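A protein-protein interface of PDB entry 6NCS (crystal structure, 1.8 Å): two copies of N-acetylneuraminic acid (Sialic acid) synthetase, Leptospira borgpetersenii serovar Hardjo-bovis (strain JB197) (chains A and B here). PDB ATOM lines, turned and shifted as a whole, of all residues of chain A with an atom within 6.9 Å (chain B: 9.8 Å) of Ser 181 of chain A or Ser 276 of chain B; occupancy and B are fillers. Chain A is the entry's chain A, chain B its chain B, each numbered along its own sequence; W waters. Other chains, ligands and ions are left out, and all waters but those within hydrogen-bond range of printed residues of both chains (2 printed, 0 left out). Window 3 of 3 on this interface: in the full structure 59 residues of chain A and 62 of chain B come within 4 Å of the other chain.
The side-chain carboxylate (OE2) of Glu 277 of chain B is in hydrogen-bond range of the backbone NH (N) of Gln 274 of chain B.
Val 179 of chain A touches Glu 277 of chain B (CA to OE1, 3.5 Å). CG of Glu 280 of chain B touches CB of Ser 180 of chain A, 3.6 Å away.
Water W1 lies within hydrogen-bond range of O of Ser 180 of chain A, O of Ser 276 of chain B and N of Glu 280 of chain B. Water W2 bridges the backbone carbonyl oxygen (O) of Cys 178 of chain A (2.9 Å) and the side-chain carboxylate (OE2) of Glu 277 of chain B (2.9 Å).
Ser 181 of chain A touches just one residue of chain B: Ser 276. Of chain B, only Glu 277 and Glu 280 come within 4 Å of Ser 180 of chain A. Tyr 182 of chain A touches none of the printed residues of chain B. Of the printed residues of chain B, Asp 188 of chain A touches Gln 274 and Ser 276. Of the printed residues of chain B, Val 179 of chain A touches Glu 277. Printed residues of chain A within 4 Å of Gln 274 of chain B: Asp 188 (3.4 Å). Cys 178 of chain A touches none of the printed residues of chain B. The nearest printed residue of chain A that does not touch Glu 277 of chain B is Cys 178 of chain A (4.1 Å).
OE1 of Glu 277 of chain B sits at hydrogen-bond distance from N of Ser 180 of chain A (2.8 Å). The side-chain hydroxyl of Ser 276 of chain B lies within hydrogen-bond range of the side-chain hydroxyl of Ser 181 of chain A (3.1 Å). The side-chain carboxylate of Asp 188 of chain A lies close to the side-chain amide oxygen of Gln 274 of chain B. OG of Ser 276 of chain B is in hydrogen-bond range of OD2 of Asp 188 of chain A, 2.8 Å away.
Hydrophobic or aromatic side chains of chain A within 4 Å of the printed part of chain B: Val 179. Along chain A the printed residues that touch a printed residue of chain B span positions 179 to 188. Printed residues of chain B that touch a printed residue of chain A: Gln 274, Ser 276, Glu 277 and Glu 280. Among the printed residues, no Asp or Glu carboxylate lies within 4 Å of a Lys or Arg side-chain nitrogen of the other chain.
No position is printed for both chains.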
ATOM      1  N   CYS A 178      32.093  33.799  18.490  1.00  0.00           N
ATOM      2  CA  CYS A 178      31.443  32.985  19.501  1.00  0.00           C
ATOM      3  C   CYS A 178      30.623  31.934  18.771  1.00  0.00           C
ATOM      4  O   CYS A 178      30.139  32.182  17.662  1.00  0.00           O
ATOM      5  CB  CYS A 178      30.537  33.851  20.403  1.00  0.00           C
ATOM      6  SG  CYS A 178      29.749  32.958  21.756  1.00  0.00           S
ATOM      7  N   VAL A 179      30.499  30.757  19.377  1.00  0.00           N
ATOM      8  CA  VAL A 179      29.659  29.690  18.848  1.00  0.00           C
ATOM      9  C   VAL A 179      28.706  29.270  19.955  1.00  0.00           C
ATOM     10  O   VAL A 179      29.150  28.772  20.997  1.00  0.00           O
ATOM     11  CB  VAL A 179      30.483  28.485  18.356  1.00  0.00           C
ATOM     12  CG1 VAL A 179      29.567  27.378  17.835  1.00  0.00           C
ATOM     13  CG2 VAL A 179      31.469  28.932  17.294  1.00  0.00           C
ATOM     14  N   SER A 180      27.402  29.488  19.736  1.00  0.00           N
ATOM     15  CA  SER A 180      26.363  29.177  20.719  1.00  0.00           C
ATOM     16  C   SER A 180      26.011  27.691  20.694  1.00  0.00           C
ATOM     17  O   SER A 180      24.881  27.283  20.414  1.00  0.00           O
ATOM     18  CB  SER A 180      25.127  30.033  20.474  1.00  0.00           C
ATOM     19  OG  SER A 180      25.434  31.407  20.632  1.00  0.00           O
ATOM     20  N   SER A 181      27.018  26.880  21.016  1.00  0.00           N
ATOM     21  CA  SER A 181      26.891  25.437  21.154  1.00  0.00           C
ATOM     22  C   SER A 181      27.343  25.042  22.557  1.00  0.00           C
ATOM     23  O   SER A 181      28.351  25.547  23.056  1.00  0.00           O
ATOM     24  CB  SER A 181      27.731  24.720  20.085  1.00  0.00           C
ATOM     25  OG  SER A 181      27.587  23.318  20.168  1.00  0.00           O
ATOM     26  N   TYR A 182      26.608  24.141  23.199  1.00  0.00           N
ATOM     27  CA  TYR A 182      26.830  23.844  24.616  1.00  0.00           C
ATOM     28  C   TYR A 182      26.875  22.343  24.866  1.00  0.00           C
ATOM     29  O   TYR A 182      25.828  21.670  24.770  1.00  0.00           O
ATOM     30  CB  TYR A 182      25.752  24.515  25.465  1.00  0.00           C
ATOM     31  CG  TYR A 182      25.798  26.027  25.365  1.00  0.00           C
ATOM     32  CD1 TYR A 182      25.125  26.700  24.349  1.00  0.00           C
ATOM     33  CD2 TYR A 182      26.532  26.780  26.273  1.00  0.00           C
ATOM     34  CE1 TYR A 182      25.178  28.082  24.244  1.00  0.00           C
ATOM     35  CE2 TYR A 182      26.587  28.164  26.178  1.00  0.00           C
ATOM     36  CZ  TYR A 182      25.913  28.806  25.160  1.00  0.00           C
ATOM     37  OH  TYR A 182      25.967  30.178  25.063  1.00  0.00           O
ATOM     38  N   PRO A 183      28.052  21.768  25.160  1.00  0.00           N
ATOM     39  CA  PRO A 183      29.338  22.471  25.082  1.00  0.00           C
ATOM     40  C   PRO A 183      29.834  22.540  23.643  1.00  0.00           C
ATOM     41  O   PRO A 183      29.385  21.764  22.797  1.00  0.00           O
ATOM     42  CB  PRO A 183      30.262  21.606  25.944  1.00  0.00           C
ATOM     43  CG  PRO A 183      29.692  20.238  25.837  1.00  0.00           C
ATOM     44  CD  PRO A 183      28.201  20.393  25.678  1.00  0.00           C
ATOM     45  N   MET A 184      30.757  23.452  23.367  1.00  0.00           N
ATOM     46  CA  MET A 184      31.232  23.645  22.003  1.00  0.00           C
ATOM     47  C   MET A 184      32.339  22.641  21.709  1.00  0.00           C
ATOM     48  O   MET A 184      33.332  22.564  22.442  1.00  0.00           O
ATOM     49  CB  MET A 184      31.728  25.073  21.795  1.00  0.00           C
ATOM     50  CG  MET A 184      32.029  25.379  20.338  1.00  0.00           C
ATOM     51  SD  MET A 184      33.175  26.736  20.150  1.00  0.00           S
ATOM     52  CE  MET A 184      34.647  25.943  20.815  1.00  0.00           C
ATOM     53  N   ASN A 185      32.162  21.865  20.645  1.00  0.00           N
ATOM     54  CA  ASN A 185      33.159  20.888  20.239  1.00  0.00           C
ATOM     55  C   ASN A 185      34.236  21.552  19.380  1.00  0.00           C
ATOM     56  O   ASN A 185      34.021  22.603  18.780  1.00  0.00           O
ATOM     57  CB  ASN A 185      32.494  19.746  19.479  1.00  0.00           C
ATOM     58  CG  ASN A 185      31.377  19.088  20.277  1.00  0.00           C
ATOM     59  OD1 ASN A 185      31.549  18.758  21.453  1.00  0.00           O
ATOM     60  ND2 ASN A 185      30.221  18.911  19.645  1.00  0.00           N
ATOM     61  N   ASP A 188      33.655  22.776  15.807  1.00  0.00           N
ATOM     62  CA  ASP A 188      32.700  23.863  15.649  1.00  0.00           C
ATOM     63  C   ASP A 188      33.287  25.236  15.954  1.00  0.00           C
ATOM     64  O   ASP A 188      32.582  26.231  15.803  1.00  0.00           O
ATOM     65  CB  ASP A 188      31.483  23.636  16.552  1.00  0.00           C
ATOM     66  CG  ASP A 188      30.538  22.587  16.009  1.00  0.00           C
ATOM     67  OD1 ASP A 188      30.513  22.385  14.775  1.00  0.00           O
ATOM     68  OD2 ASP A 188      29.814  21.969  16.820  1.00  0.00           O
ATOM     69  N   HIS A 210      32.964  28.609  24.770  1.00  0.00           N
ATOM     70  CA  HIS A 210      32.005  27.729  25.430  1.00  0.00           C
ATOM     71  C   HIS A 210      32.467  26.277  25.362  1.00  0.00           C
ATOM     72  O   HIS A 210      31.652  25.348  25.385  1.00  0.00           O
ATOM     73  CB  HIS A 210      30.611  27.914  24.839  1.00  0.00           C
ATOM     74  CG  HIS A 210      30.066  29.282  25.082  1.00  0.00           C
ATOM     75  ND1 HIS A 210      30.170  30.301  24.159  1.00  0.00           N
ATOM     76  CD2 HIS A 210      29.493  29.827  26.182  1.00  0.00           C
ATOM     77  CE1 HIS A 210      29.641  31.403  24.663  1.00  0.00           C
ATOM     78  NE2 HIS A 210      29.225  31.142  25.890  1.00  0.00           N
ATOM     79  N   SER A 211      33.777  26.076  25.295  1.00  0.00           N
ATOM     80  CA  SER A 211      34.363  24.749  25.322  1.00  0.00           C
ATOM     81  C   SER A 211      34.636  24.310  26.757  1.00  0.00           C
ATOM     82  O   SER A 211      34.541  25.089  27.708  1.00  0.00           O
ATOM     83  CB  SER A 211      35.671  24.723  24.537  1.00  0.00           C
ATOM     84  OG  SER A 211      36.705  25.254  25.345  1.00  0.00           O
ATOM     85  N   ILE A 245      31.379  23.962  31.297  1.00  0.00           N
ATOM     86  CA  ILE A 245      32.196  24.774  30.395  1.00  0.00           C
ATOM     87  C   ILE A 245      32.990  25.842  31.139  1.00  0.00           C
ATOM     88  O   ILE A 245      33.537  26.751  30.504  1.00  0.00           O
ATOM     89  CB  ILE A 245      31.348  25.413  29.285  1.00  0.00           C
ATOM     90  CG1 ILE A 245      30.291  26.355  29.871  1.00  0.00           C
ATOM     91  CG2 ILE A 245      30.706  24.343  28.411  1.00  0.00           C
ATOM     92  CD1 ILE A 245      29.735  27.323  28.848  1.00  0.00           C
ATOM     93  N   GLU B 272      28.823  32.354   9.235  1.00  0.00           N
ATOM     94  CA  GLU B 272      27.539  31.692   9.230  1.00  0.00           C
ATOM     95  C   GLU B 272      27.553  30.724  10.402  1.00  0.00           C
ATOM     96  O   GLU B 272      28.610  30.149  10.710  1.00  0.00           O
ATOM     97  CB  GLU B 272      27.252  30.965   7.911  1.00  0.00           C
ATOM     98  CG  GLU B 272      28.206  29.841   7.579  1.00  0.00           C
ATOM     99  CD  GLU B 272      27.988  29.281   6.184  1.00  0.00           C
ATOM    100  OE1 GLU B 272      27.517  30.035   5.307  1.00  0.00           O
ATOM    101  OE2 GLU B 272      28.289  28.087   5.965  1.00  0.00           O
ATOM    102  N   PRO B 273      26.427  30.547  11.083  1.00  0.00           N
ATOM    103  CA  PRO B 273      26.419  29.725  12.298  1.00  0.00           C
ATOM    104  C   PRO B 273      26.704  28.255  12.014  1.00  0.00           C
ATOM    105  O   PRO B 273      26.459  27.746  10.917  1.00  0.00           O
ATOM    106  CB  PRO B 273      24.997  29.921  12.840  1.00  0.00           C
ATOM    107  CG  PRO B 273      24.182  30.263  11.626  1.00  0.00           C
ATOM    108  CD  PRO B 273      25.099  31.105  10.776  1.00  0.00           C
ATOM    109  N   GLN B 274      27.238  27.570  13.026  1.00  0.00           N
ATOM    110  CA  GLN B 274      27.415  26.124  12.946  1.00  0.00           C
ATOM    111  C   GLN B 274      26.079  25.412  13.152  1.00  0.00           C
ATOM    112  O   GLN B 274      25.173  25.923  13.817  1.00  0.00           O
ATOM    113  CB  GLN B 274      28.429  25.646  13.990  1.00  0.00           C
ATOM    114  CG  GLN B 274      29.777  26.371  13.944  1.00  0.00           C
ATOM    115  CD  GLN B 274      30.615  25.971  12.741  1.00  0.00           C
ATOM    116  OE1 GLN B 274      30.713  24.791  12.399  1.00  0.00           O
ATOM    117  NE2 GLN B 274      31.221  26.957  12.093  1.00  0.00           N
ATOM    118  N   ALA B 275      25.962  24.213  12.569  1.00  0.00           N
ATOM    119  CA  ALA B 275      24.743  23.420  12.716  1.00  0.00           C
ATOM    120  C   ALA B 275      24.369  23.220  14.183  1.00  0.00           C
ATOM    121  O   ALA B 275      23.184  23.239  14.544  1.00  0.00           O
ATOM    122  CB  ALA B 275      24.929  22.070  12.031  1.00  0.00           C
ATOM    123  N   SER B 276      25.369  23.032  15.046  1.00  0.00           N
ATOM    124  CA  SER B 276      25.124  22.813  16.466  1.00  0.00           C
ATOM    125  C   SER B 276      24.540  24.030  17.176  1.00  0.00           C
ATOM    126  O   SER B 276      24.110  23.898  18.325  1.00  0.00           O
ATOM    127  CB  SER B 276      26.419  22.399  17.163  1.00  0.00           C
ATOM    128  OG  SER B 276      27.383  23.427  17.061  1.00  0.00           O
ATOM    129  N   GLU B 277      24.527  25.205  16.546  1.00  0.00           N
ATOM    130  CA  GLU B 277      23.924  26.387  17.158  1.00  0.00           C
ATOM    131  C   GLU B 277      22.409  26.443  16.966  1.00  0.00           C
ATOM    132  O   GLU B 277      21.782  27.433  17.357  1.00  0.00           O
ATOM    133  CB  GLU B 277      24.575  27.658  16.596  1.00  0.00           C
ATOM    134  CG  GLU B 277      26.066  27.791  16.937  1.00  0.00           C
ATOM    135  CD  GLU B 277      26.702  29.099  16.443  1.00  0.00           C
ATOM    136  OE1 GLU B 277      26.646  30.124  17.167  1.00  0.00           O
ATOM    137  OE2 GLU B 277      27.280  29.093  15.331  1.00  0.00           O
ATOM    138  N   GLN B 278      21.807  25.384  16.415  1.00  0.00           N
ATOM    139  CA  GLN B 278      20.408  25.443  15.991  1.00  0.00           C
ATOM    140  C   GLN B 278      19.456  25.688  17.162  1.00  0.00           C
ATOM    141  O   GLN B 278      18.501  26.465  17.039  1.00  0.00           O
ATOM    142  CB  GLN B 278      20.035  24.155  15.257  1.00  0.00           C
ATOM    143  CG  GLN B 278      18.615  24.153  14.726  1.00  0.00           C
ATOM    144  CD  GLN B 278      18.310  25.368  13.866  1.00  0.00           C
ATOM    145  OE1 GLN B 278      19.171  25.869  13.141  1.00  0.00           O
ATOM    146  NE2 GLN B 278      17.077  25.853  13.949  1.00  0.00           N
ATOM    147  N   GLU B 279      19.693  25.032  18.301  1.00  0.00           N
ATOM    148  CA  GLU B 279      18.852  25.252  19.476  1.00  0.00           C
ATOM    149  C   GLU B 279      18.846  26.718  19.883  1.00  0.00           C
ATOM    150  O   GLU B 279      17.793  27.288  20.200  1.00  0.00           O
ATOM    151  CB  GLU B 279      19.338  24.400  20.648  1.00  0.00           C
ATOM    152  CG  GLU B 279      18.734  23.021  20.751  1.00  0.00           C
ATOM    153  CD  GLU B 279      18.844  22.464  22.157  1.00  0.00           C
ATOM    154  OE1 GLU B 279      17.869  22.597  22.928  1.00  0.00           O
ATOM    155  OE2 GLU B 279      19.912  21.911  22.497  1.00  0.00           O
ATOM    156  N   GLU B 280      20.023  27.342  19.905  1.00  0.00           N
ATOM    157  CA  GLU B 280      20.104  28.722  20.365  1.00  0.00           C
ATOM    158  C   GLU B 280      19.516  29.687  19.345  1.00  0.00           C
ATOM    159  O   GLU B 280      18.947  30.719  19.726  1.00  0.00           O
ATOM    160  CB  GLU B 280      21.555  29.080  20.679  1.00  0.00           C
ATOM    161  CG  GLU B 280      21.714  30.402  21.424  1.00  0.00           C
ATOM    162  CD  GLU B 280      21.352  30.303  22.898  1.00  0.00           C
ATOM    163  OE1 GLU B 280      21.411  31.343  23.591  1.00  0.00           O
ATOM    164  OE2 GLU B 280      21.020  29.193  23.364  1.00  0.00           O
ATOM    165  N   ILE B 281      19.639  29.368  18.053  1.00  0.00           N
ATOM    166  CA  ILE B 281      18.994  30.166  17.013  1.00  0.00           C
ATOM    167  C   ILE B 281      17.481  30.160  17.191  1.00  0.00           C
ATOM    168  O   ILE B 281      16.825  31.202  17.079  1.00  0.00           O
ATOM    169  CB  ILE B 281      19.396  29.655  15.617  1.00  0.00           C
ATOM    170  CG1 ILE B 281      20.871  29.981  15.337  1.00  0.00           C
ATOM    171  CG2 ILE B 281      18.489  30.260  14.554  1.00  0.00           C
ATOM    172  CD1 ILE B 281      21.439  29.262  14.131  1.00  0.00           C
ATOM    173  N   GLU B 282      16.898  28.987  17.459  1.00  0.00           N
ATOM    174  CA  GLU B 282      15.447  28.906  17.614  1.00  0.00           C
ATOM    175  C   GLU B 282      14.979  29.653  18.856  1.00  0.00           C
ATOM    176  O   GLU B 282      13.928  30.307  18.837  1.00  0.00           O
ATOM    177  CB  GLU B 282      15.002  27.449  17.672  1.00  0.00           C
ATOM    178  CG  GLU B 282      15.241  26.699  16.388  1.00  0.00           C
ATOM    179  CD  GLU B 282      14.880  25.235  16.491  1.00  0.00           C
ATOM    180  OE1 GLU B 282      14.052  24.881  17.360  1.00  0.00           O
ATOM    181  OE2 GLU B 282      15.433  24.439  15.704  1.00  0.00           O
HETATM  182  O   HOH W   1      22.795  25.674  20.259  1.00  0.00           O
HETATM  183  O   HOH W   2      29.270  31.249  15.094  1.00  0.00           O
